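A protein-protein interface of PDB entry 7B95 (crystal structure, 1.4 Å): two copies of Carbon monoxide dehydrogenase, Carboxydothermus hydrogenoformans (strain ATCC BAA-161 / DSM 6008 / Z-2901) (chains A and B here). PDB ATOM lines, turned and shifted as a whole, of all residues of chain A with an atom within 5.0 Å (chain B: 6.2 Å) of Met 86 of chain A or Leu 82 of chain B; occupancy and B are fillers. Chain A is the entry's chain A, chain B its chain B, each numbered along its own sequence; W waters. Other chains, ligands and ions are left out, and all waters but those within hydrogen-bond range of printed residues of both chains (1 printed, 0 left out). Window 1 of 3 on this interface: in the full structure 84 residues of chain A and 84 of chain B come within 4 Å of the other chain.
Among the printed residues, merely in contact across the chains: Leu 82 of chain A with Met 86 of chain B, Met 86 of chain A with Leu 82 of chain B, Met 86 of chain A with Ala 191 of chain B, Gly 87 of chain A with Leu 195 of chain B, Ser 89 of chain A with Ala 191 of chain B, Ser 89 of chain A with Ala 192 of chain B, Thr 90 of chain A with Ala 192 of chain B and Gln 557 of chain A with Leu 195 of chain B.
Of chain B, only Leu 82 (3.8 Å), Ala 191 (3.4 Å), Cys 194 (3.5 Å) and Leu 195 (3.6 Å) come within 4 Å of Met 86 of chain A.
Leu 82 of chain B touches just one residue of chain A: Met 86.
Printed residues of chain B within 4 Å of Gly 87 of chain A: Leu 195 (3.95 Å).
Printed residues of chain A within 4 Å of Ala 192 of chain B: Ser 89 (3.9 Å) and Thr 90 (3.9 Å).
Printed residues of chain B within 4 Å of Ser 89 of chain A: Ala 191 and Ala 192.
Of the printed residues of chain B, Leu 82 of chain A touches Met 86 (3.7 Å).
Along chain B the printed residues that touch a printed residue of chain A span positions 49 to 195.
Along chain A the printed residues that touch a printed residue of chain B span positions 82 to 557.
Among the printed residues, 11 pairs touch across the chains.
Among the printed residues, no Asp or Glu carboxylate lies within 4 Å of a Lys or Arg side-chain nitrogen of the other chain.
SD of Met 86 of chain A lies close to O of Cys 194 of chain B, 3.5 Å away.
O of Leu 49 of chain B sits at hydrogen-bond distance from NE2 of Gln 557 of chain A (2.9 Å).
SD of Met 86 of chain A lies within hydrogen-bond range of N of Leu 195 of chain B, 3.6 Å away.
Leu 82 of chain A touches Met 86 of chain B, and with the chains exchanged Met 86 of chain A touches Leu 82 of chain B.
6 positions are printed for both chains.
Of the 11 pairs that touch across the chains among the printed residues, 2 have their exchanged pair printed and touching as well.
Water W1 lies within hydrogen-bond range of OG1 of Thr 196 of chain B (2.8 Å), OE1 of Gln 557 of chain A (2.8 Å) and O of Leu 49 of chain B (2.9 Å).
The side-chain sulfur (SG) of Cys 194 of chain B sits at hydrogen-bond distance from the backbone carbonyl oxygen (O) of Ala 190 of chain B (3.4 Å).
OG1 of Thr 90 of chain A lies within hydrogen-bond range of O of Gly 87 of chain A, at 2.8 Å.
The backbone carbonyl oxygen (O) of Val 85 of chain A lies within hydrogen-bond range of the side-chain hydroxyl (OG) of Ser 89 of chain A (2.8 Å).
The side-chain sulfur (SG) of Cys 194 of chain B is in hydrogen-bond range of the backbone carbonyl oxygen (O) of Arg 78 of chain B (3.4 Å).
The side-chain sulfur of Cys 194 of chain B lies within hydrogen-bond range of the backbone NH of Leu 82 of chain B, 3.7 Å away.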
ATOM      1  N   LEU A  82     -15.732 -16.347  25.464  1.00  0.00           N
ATOM      2  CA  LEU A  82     -15.159 -16.396  24.120  1.00  0.00           C
ATOM      3  C   LEU A  82     -16.220 -16.794  23.108  1.00  0.00           C
ATOM      4  O   LEU A  82     -16.324 -16.201  22.033  1.00  0.00           O
ATOM      5  CB  LEU A  82     -14.003 -17.404  24.091  1.00  0.00           C
ATOM      6  CG  LEU A  82     -13.367 -17.626  22.704  1.00  0.00           C
ATOM      7  CD1 LEU A  82     -12.797 -16.331  22.104  1.00  0.00           C
ATOM      8  CD2 LEU A  82     -12.316 -18.739  22.784  1.00  0.00           C
ATOM      9  N   ARG A  83     -17.009 -17.833  23.421  1.00  0.00           N
ATOM     10  CA  ARG A  83     -18.053 -18.218  22.475  1.00  0.00           C
ATOM     11  C   ARG A  83     -19.063 -17.097  22.286  1.00  0.00           C
ATOM     12  O   ARG A  83     -19.582 -16.905  21.180  1.00  0.00           O
ATOM     13  CB  ARG A  83     -18.742 -19.518  22.928  1.00  0.00           C
ATOM     14  CG  ARG A  83     -17.829 -20.745  22.790  1.00  0.00           C
ATOM     15  CD  ARG A  83     -18.553 -22.052  23.192  1.00  0.00           C
ATOM     16  NE  ARG A  83     -18.681 -22.020  24.628  1.00  0.00           N
ATOM     17  CZ  ARG A  83     -18.305 -22.951  25.486  1.00  0.00           C
ATOM     18  NH1 ARG A  83     -17.943 -24.153  25.131  1.00  0.00           N
ATOM     19  NH2 ARG A  83     -18.409 -22.688  26.763  1.00  0.00           N
ATOM     20  N   ASN A  84     -19.325 -16.329  23.346  1.00  0.00           N
ATOM     21  CA  ASN A  84     -20.267 -15.227  23.246  1.00  0.00           C
ATOM     22  C   ASN A  84     -19.727 -14.070  22.439  1.00  0.00           C
ATOM     23  O   ASN A  84     -20.513 -13.254  21.962  1.00  0.00           O
ATOM     24  CB  ASN A  84     -20.799 -14.816  24.617  1.00  0.00           C
ATOM     25  CG  ASN A  84     -21.950 -15.707  25.039  1.00  0.00           C
ATOM     26  OD1 ASN A  84     -23.099 -15.459  24.698  1.00  0.00           O
ATOM     27  ND2 ASN A  84     -21.628 -16.843  25.653  1.00  0.00           N
ATOM     28  N   VAL A  85     -18.415 -13.996  22.247  1.00  0.00           N
ATOM     29  CA  VAL A  85     -17.879 -13.076  21.256  1.00  0.00           C
ATOM     30  C   VAL A  85     -18.428 -13.407  19.874  1.00  0.00           C
ATOM     31  O   VAL A  85     -18.698 -12.509  19.074  1.00  0.00           O
ATOM     32  CB  VAL A  85     -16.342 -13.077  21.300  1.00  0.00           C
ATOM     33  CG1 VAL A  85     -15.725 -12.355  20.108  1.00  0.00           C
ATOM     34  CG2 VAL A  85     -15.832 -12.435  22.607  1.00  0.00           C
ATOM     35  N   MET A  86     -18.584 -14.702  19.555  1.00  0.00           N
ATOM     36  CA  MET A  86     -19.172 -15.064  18.268  1.00  0.00           C
ATOM     37  C   MET A  86     -20.600 -14.556  18.165  1.00  0.00           C
ATOM     38  O   MET A  86     -21.011 -14.038  17.133  1.00  0.00           O
ATOM     39  CB  MET A  86     -19.171 -16.580  18.051  1.00  0.00           C
ATOM     40  CG  MET A  86     -17.796 -17.224  18.089  1.00  0.00           C
ATOM     41  SD  MET A  86     -17.805 -18.952  17.579  1.00  0.00           S
ATOM     42  CE  MET A  86     -18.637 -19.727  18.963  1.00  0.00           C
ATOM     43  N   GLY A  87     -21.391 -14.769  19.212  1.00  0.00           N
ATOM     44  CA  GLY A  87     -22.773 -14.329  19.183  1.00  0.00           C
ATOM     45  C   GLY A  87     -22.875 -12.837  18.972  1.00  0.00           C
ATOM     46  O   GLY A  87     -23.657 -12.377  18.140  1.00  0.00           O
ATOM     47  N   THR A  88     -22.098 -12.060  19.737  1.00  0.00           N
ATOM     48  CA  THR A  88     -22.125 -10.606  19.612  1.00  0.00           C
ATOM     49  C   THR A  88     -21.649 -10.189  18.231  1.00  0.00           C
ATOM     50  O   THR A  88     -22.173  -9.243  17.643  1.00  0.00           O
ATOM     51  CB  THR A  88     -21.249  -9.945  20.690  1.00  0.00           C
ATOM     52  OG1 THR A  88     -21.631 -10.405  21.982  1.00  0.00           O
ATOM     53  CG2 THR A  88     -21.431  -8.447  20.650  1.00  0.00           C
ATOM     54  N   SER A  89     -20.628 -10.871  17.714  1.00  0.00           N
ATOM     55  CA  SER A  89     -20.109 -10.527  16.394  1.00  0.00           C
ATOM     56  C   SER A  89     -21.165 -10.692  15.311  1.00  0.00           C
ATOM     57  O   SER A  89     -21.199  -9.905  14.355  1.00  0.00           O
ATOM     58  CB  SER A  89     -18.862 -11.361  16.043  1.00  0.00           C
ATOM     59  OG  SER A  89     -17.768 -11.024  16.865  1.00  0.00           O
ATOM     60  N   THR A  90     -21.982 -11.745  15.388  1.00  0.00           N
ATOM     61  CA  THR A  90     -23.031 -11.917  14.385  1.00  0.00           C
ATOM     62  C   THR A  90     -24.041 -10.785  14.433  1.00  0.00           C
ATOM     63  O   THR A  90     -24.440 -10.258  13.387  1.00  0.00           O
ATOM     64  CB  THR A  90     -23.747 -13.271  14.499  1.00  0.00           C
ATOM     65  OG1 THR A  90     -24.562 -13.353  15.667  1.00  0.00           O
ATOM     66  CG2 THR A  90     -22.794 -14.384  14.488  1.00  0.00           C
ATOM     67  N   GLN A 557     -24.651 -19.093  20.528  1.00  0.00           N
ATOM     68  CA  GLN A 557     -24.462 -17.962  21.417  1.00  0.00           C
ATOM     69  C   GLN A 557     -25.172 -16.679  20.992  1.00  0.00           C
ATOM     70  O   GLN A 557     -25.045 -15.664  21.684  1.00  0.00           O
ATOM     71  CB  GLN A 557     -22.977 -17.724  21.645  1.00  0.00           C
ATOM     72  CG  GLN A 557     -22.277 -18.906  22.269  1.00  0.00           C
ATOM     73  CD  GLN A 557     -22.042 -20.051  21.284  1.00  0.00           C
ATOM     74  OE1 GLN A 557     -21.889 -19.811  20.082  1.00  0.00           O
ATOM     75  NE2 GLN A 557     -21.983 -21.266  21.777  1.00  0.00           N
ATOM     76  N   LEU B  49     -18.619 -25.878  20.424  1.00  0.00           N
ATOM     77  CA  LEU B  49     -19.174 -24.589  20.030  1.00  0.00           C
ATOM     78  C   LEU B  49     -20.693 -24.483  20.083  1.00  0.00           C
ATOM     79  O   LEU B  49     -21.202 -23.358  19.973  1.00  0.00           O
ATOM     80  CB  LEU B  49     -18.675 -24.180  18.645  1.00  0.00           C
ATOM     81  CG  LEU B  49     -17.170 -24.007  18.515  1.00  0.00           C
ATOM     82  CD1 LEU B  49     -16.822 -23.434  17.183  1.00  0.00           C
ATOM     83  CD2 LEU B  49     -16.576 -23.138  19.631  1.00  0.00           C
ATOM     84  N   MET B  77      -9.912 -26.215  11.691  1.00  0.00           N
ATOM     85  CA  MET B  77      -9.554 -24.876  11.233  1.00  0.00           C
ATOM     86  C   MET B  77     -10.435 -23.808  11.895  1.00  0.00           C
ATOM     87  O   MET B  77      -9.970 -22.699  12.190  1.00  0.00           O
ATOM     88  CB  MET B  77      -9.609 -24.786   9.714  1.00  0.00           C
ATOM     89  CG  MET B  77      -9.038 -23.459   9.164  1.00  0.00           C
ATOM     90  SD  MET B  77      -7.280 -23.242   9.525  1.00  0.00           S
ATOM     91  CE  MET B  77      -7.307 -21.621  10.328  1.00  0.00           C
ATOM     92  N   ARG B  78     -11.703 -24.122  12.153  1.00  0.00           N
ATOM     93  CA  ARG B  78     -12.602 -23.148  12.752  1.00  0.00           C
ATOM     94  C   ARG B  78     -12.150 -22.809  14.168  1.00  0.00           C
ATOM     95  O   ARG B  78     -12.156 -21.639  14.552  1.00  0.00           O
ATOM     96  CB  ARG B  78     -14.031 -23.702  12.754  1.00  0.00           C
ATOM     97  CG  ARG B  78     -15.061 -22.752  13.367  1.00  0.00           C
ATOM     98  CD  ARG B  78     -16.452 -23.258  13.162  1.00  0.00           C
ATOM     99  NE  ARG B  78     -16.627 -24.555  13.813  1.00  0.00           N
ATOM    100  CZ  ARG B  78     -17.786 -25.217  13.844  1.00  0.00           C
ATOM    101  NH1 ARG B  78     -18.854 -24.727  13.223  1.00  0.00           N
ATOM    102  NH2 ARG B  78     -17.859 -26.400  14.454  1.00  0.00           N
ATOM    103  N   TYR B  79     -11.774 -23.808  14.975  1.00  0.00           N
ATOM    104  CA  TYR B  79     -11.345 -23.490  16.329  1.00  0.00           C
ATOM    105  C   TYR B  79     -10.028 -22.735  16.296  1.00  0.00           C
ATOM    106  O   TYR B  79      -9.819 -21.820  17.099  1.00  0.00           O
ATOM    107  CB  TYR B  79     -11.322 -24.743  17.201  1.00  0.00           C
ATOM    108  CG  TYR B  79     -11.304 -24.580  18.701  1.00  0.00           C
ATOM    109  CD1 TYR B  79     -11.440 -23.353  19.329  1.00  0.00           C
ATOM    110  CD2 TYR B  79     -11.188 -25.691  19.497  1.00  0.00           C
ATOM    111  CE1 TYR B  79     -11.440 -23.269  20.718  1.00  0.00           C
ATOM    112  CE2 TYR B  79     -11.194 -25.623  20.868  1.00  0.00           C
ATOM    113  CZ  TYR B  79     -11.345 -24.405  21.483  1.00  0.00           C
ATOM    114  OH  TYR B  79     -11.325 -24.298  22.856  1.00  0.00           O
ATOM    115  N   MET B  80      -9.130 -23.082  15.372  1.00  0.00           N
ATOM    116  CA  MET B  80      -7.929 -22.275  15.187  1.00  0.00           C
ATOM    117  C   MET B  80      -8.272 -20.824  14.870  1.00  0.00           C
ATOM    118  O   MET B  80      -7.712 -19.902  15.457  1.00  0.00           O
ATOM    119  CB  MET B  80      -7.080 -22.858  14.074  1.00  0.00           C
ATOM    120  CG  MET B  80      -5.919 -21.992  13.649  1.00  0.00           C
ATOM    121  SD  MET B  80      -4.714 -22.839  12.639  1.00  0.00           S
ATOM    122  CE  MET B  80      -4.632 -24.437  13.422  1.00  0.00           C
ATOM    123  N   LEU B  81      -9.213 -20.607  13.967  1.00  0.00           N
ATOM    124  CA  LEU B  81      -9.588 -19.246  13.614  1.00  0.00           C
ATOM    125  C   LEU B  81     -10.167 -18.514  14.808  1.00  0.00           C
ATOM    126  O   LEU B  81      -9.809 -17.352  15.068  1.00  0.00           O
ATOM    127  CB  LEU B  81     -10.585 -19.261  12.462  1.00  0.00           C
ATOM    128  CG  LEU B  81     -10.991 -17.894  11.888  1.00  0.00           C
ATOM    129  CD1 LEU B  81      -9.790 -17.163  11.318  1.00  0.00           C
ATOM    130  CD2 LEU B  81     -12.017 -18.022  10.765  1.00  0.00           C
ATOM    131  N   LEU B  82     -11.052 -19.178  15.560  1.00  0.00           N
ATOM    132  CA  LEU B  82     -11.652 -18.536  16.727  1.00  0.00           C
ATOM    133  C   LEU B  82     -10.585 -18.139  17.737  1.00  0.00           C
ATOM    134  O   LEU B  82     -10.604 -17.027  18.272  1.00  0.00           O
ATOM    135  CB  LEU B  82     -12.679 -19.463  17.390  1.00  0.00           C
ATOM    136  CG  LEU B  82     -13.296 -18.917  18.703  1.00  0.00           C
ATOM    137  CD1 LEU B  82     -14.054 -17.607  18.436  1.00  0.00           C
ATOM    138  CD2 LEU B  82     -14.207 -19.969  19.287  1.00  0.00           C
ATOM    139  N   ARG B  83      -9.647 -19.035  18.032  1.00  0.00           N
ATOM    140  CA  ARG B  83      -8.607 -18.655  18.978  1.00  0.00           C
ATOM    141  C   ARG B  83      -7.761 -17.497  18.442  1.00  0.00           C
ATOM    142  O   ARG B  83      -7.311 -16.635  19.204  1.00  0.00           O
ATOM    143  CB  ARG B  83      -7.738 -19.862  19.362  1.00  0.00           C
ATOM    144  CG  ARG B  83      -8.515 -20.900  20.191  1.00  0.00           C
ATOM    145  CD  ARG B  83      -7.636 -22.048  20.640  1.00  0.00           C
ATOM    146  NE  ARG B  83      -7.381 -22.867  19.462  1.00  0.00           N
ATOM    147  CZ  ARG B  83      -7.604 -24.167  19.306  1.00  0.00           C
ATOM    148  NH1 ARG B  83      -7.433 -24.671  18.115  1.00  0.00           N
ATOM    149  NH2 ARG B  83      -7.826 -24.988  20.309  1.00  0.00           N
ATOM    150  N   ASN B  84      -7.514 -17.481  17.133  1.00  0.00           N
ATOM    151  CA  ASN B  84      -6.745 -16.412  16.522  1.00  0.00           C
ATOM    152  C   ASN B  84      -7.485 -15.068  16.526  1.00  0.00           C
ATOM    153  O   ASN B  84      -6.845 -14.024  16.439  1.00  0.00           O
ATOM    154  CB  ASN B  84      -6.248 -16.827  15.167  1.00  0.00           C
ATOM    155  CG  ASN B  84      -4.976 -17.622  15.302  1.00  0.00           C
ATOM    156  OD1 ASN B  84      -3.882 -17.056  15.361  1.00  0.00           O
ATOM    157  ND2 ASN B  84      -5.113 -18.930  15.471  1.00  0.00           N
ATOM    158  N   VAL B  85      -8.805 -15.066  16.697  1.00  0.00           N
ATOM    159  CA  VAL B  85      -9.511 -13.828  17.005  1.00  0.00           C
ATOM    160  C   VAL B  85      -8.985 -13.231  18.316  1.00  0.00           C
ATOM    161  O   VAL B  85      -8.874 -11.996  18.445  1.00  0.00           O
ATOM    162  CB  VAL B  85     -11.036 -14.065  17.035  1.00  0.00           C
ATOM    163  CG1 VAL B  85     -11.768 -12.892  17.679  1.00  0.00           C
ATOM    164  CG2 VAL B  85     -11.560 -14.361  15.653  1.00  0.00           C
ATOM    165  N   MET B  86      -8.703 -14.067  19.327  1.00  0.00           N
ATOM    166  CA  MET B  86      -8.119 -13.540  20.557  1.00  0.00           C
ATOM    167  C   MET B  86      -6.764 -12.871  20.292  1.00  0.00           C
ATOM    168  O   MET B  86      -6.477 -11.773  20.813  1.00  0.00           O
ATOM    169  CB  MET B  86      -7.951 -14.619  21.618  1.00  0.00           C
ATOM    170  CG  MET B  86      -9.219 -15.330  22.035  1.00  0.00           C
ATOM    171  SD  MET B  86      -8.983 -16.454  23.440  1.00  0.00           S
ATOM    172  CE  MET B  86      -7.962 -17.751  22.747  1.00  0.00           C
ATOM    173  N   GLY B  87      -5.887 -13.553  19.532  1.00  0.00           N
ATOM    174  CA  GLY B  87      -4.581 -12.989  19.241  1.00  0.00           C
ATOM    175  C   GLY B  87      -4.688 -11.654  18.540  1.00  0.00           C
ATOM    176  O   GLY B  87      -4.057 -10.660  18.929  1.00  0.00           O
ATOM    177  N   ALA B 190     -14.364 -12.820  11.348  1.00  0.00           N
ATOM    178  CA  ALA B 190     -13.839 -14.146  11.620  1.00  0.00           C
ATOM    179  C   ALA B 190     -14.613 -14.808  12.750  1.00  0.00           C
ATOM    180  O   ALA B 190     -15.016 -15.977  12.638  1.00  0.00           O
ATOM    181  CB  ALA B 190     -12.367 -14.085  11.983  1.00  0.00           C
ATOM    182  N   ALA B 191     -14.896 -14.045  13.821  1.00  0.00           N
ATOM    183  CA  ALA B 191     -15.656 -14.614  14.928  1.00  0.00           C
ATOM    184  C   ALA B 191     -17.061 -15.014  14.473  1.00  0.00           C
ATOM    185  O   ALA B 191     -17.580 -16.065  14.871  1.00  0.00           O
ATOM    186  CB  ALA B 191     -15.721 -13.651  16.096  1.00  0.00           C
ATOM    187  N   ALA B 192     -17.704 -14.171  13.669  1.00  0.00           N
ATOM    188  CA  ALA B 192     -19.051 -14.501  13.196  1.00  0.00           C
ATOM    189  C   ALA B 192     -19.037 -15.748  12.315  1.00  0.00           C
ATOM    190  O   ALA B 192     -19.978 -16.551  12.341  1.00  0.00           O
ATOM    191  CB  ALA B 192     -19.635 -13.313  12.433  1.00  0.00           C
ATOM    192  N   SER B 193     -17.957 -15.927  11.540  1.00  0.00           N
ATOM    193  CA  SER B 193     -17.823 -17.088  10.679  1.00  0.00           C
ATOM    194  C   SER B 193     -17.741 -18.381  11.473  1.00  0.00           C
ATOM    195  O   SER B 193     -18.058 -19.454  10.950  1.00  0.00           O
ATOM    196  CB  SER B 193     -16.559 -16.929   9.852  1.00  0.00           C
ATOM    197  OG  SER B 193     -16.633 -15.887   8.902  1.00  0.00           O
ATOM    198  N   CYS B 194     -17.221 -18.300  12.688  1.00  0.00           N
ATOM    199  CA  CYS B 194     -17.008 -19.479  13.524  1.00  0.00           C
ATOM    200  C   CYS B 194     -18.249 -19.927  14.269  1.00  0.00           C
ATOM    201  O   CYS B 194     -18.263 -21.039  14.813  1.00  0.00           O
ATOM    202  CB  CYS B 194     -15.904 -19.231  14.551  1.00  0.00           C
ATOM    203  SG  CYS B 194     -14.247 -19.034  13.801  1.00  0.00           S
ATOM    204  N   LEU B 195     -19.287 -19.097  14.329  1.00  0.00           N
ATOM    205  CA  LEU B 195     -20.537 -19.554  14.941  1.00  0.00           C
ATOM    206  C   LEU B 195     -21.044 -20.795  14.197  1.00  0.00           C
ATOM    207  O   LEU B 195     -20.895 -20.925  12.984  1.00  0.00           O
ATOM    208  CB  LEU B 195     -21.609 -18.456  14.916  1.00  0.00           C
ATOM    209  CG  LEU B 195     -22.789 -18.682  15.833  1.00  0.00           C
ATOM    210  CD1 LEU B 195     -22.608 -17.902  17.133  1.00  0.00           C
ATOM    211  CD2 LEU B 195     -24.078 -18.327  15.159  1.00  0.00           C
ATOM    212  N   THR B 196     -21.698 -21.672  14.931  1.00  0.00           N
ATOM    213  CA  THR B 196     -22.224 -22.888  14.350  1.00  0.00           C
ATOM    214  C   THR B 196     -23.081 -22.576  13.131  1.00  0.00           C
ATOM    215  O   THR B 196     -23.893 -21.628  13.105  1.00  0.00           O
ATOM    216  CB  THR B 196     -23.021 -23.655  15.412  1.00  0.00           C
ATOM    217  OG1 THR B 196     -22.204 -23.877  16.590  1.00  0.00           O
ATOM    218  CG2 THR B 196     -23.529 -24.980  14.835  1.00  0.00           C
HETATM  219  O   HOH W   1     -21.748 -21.450  17.833  1.00  0.00           O
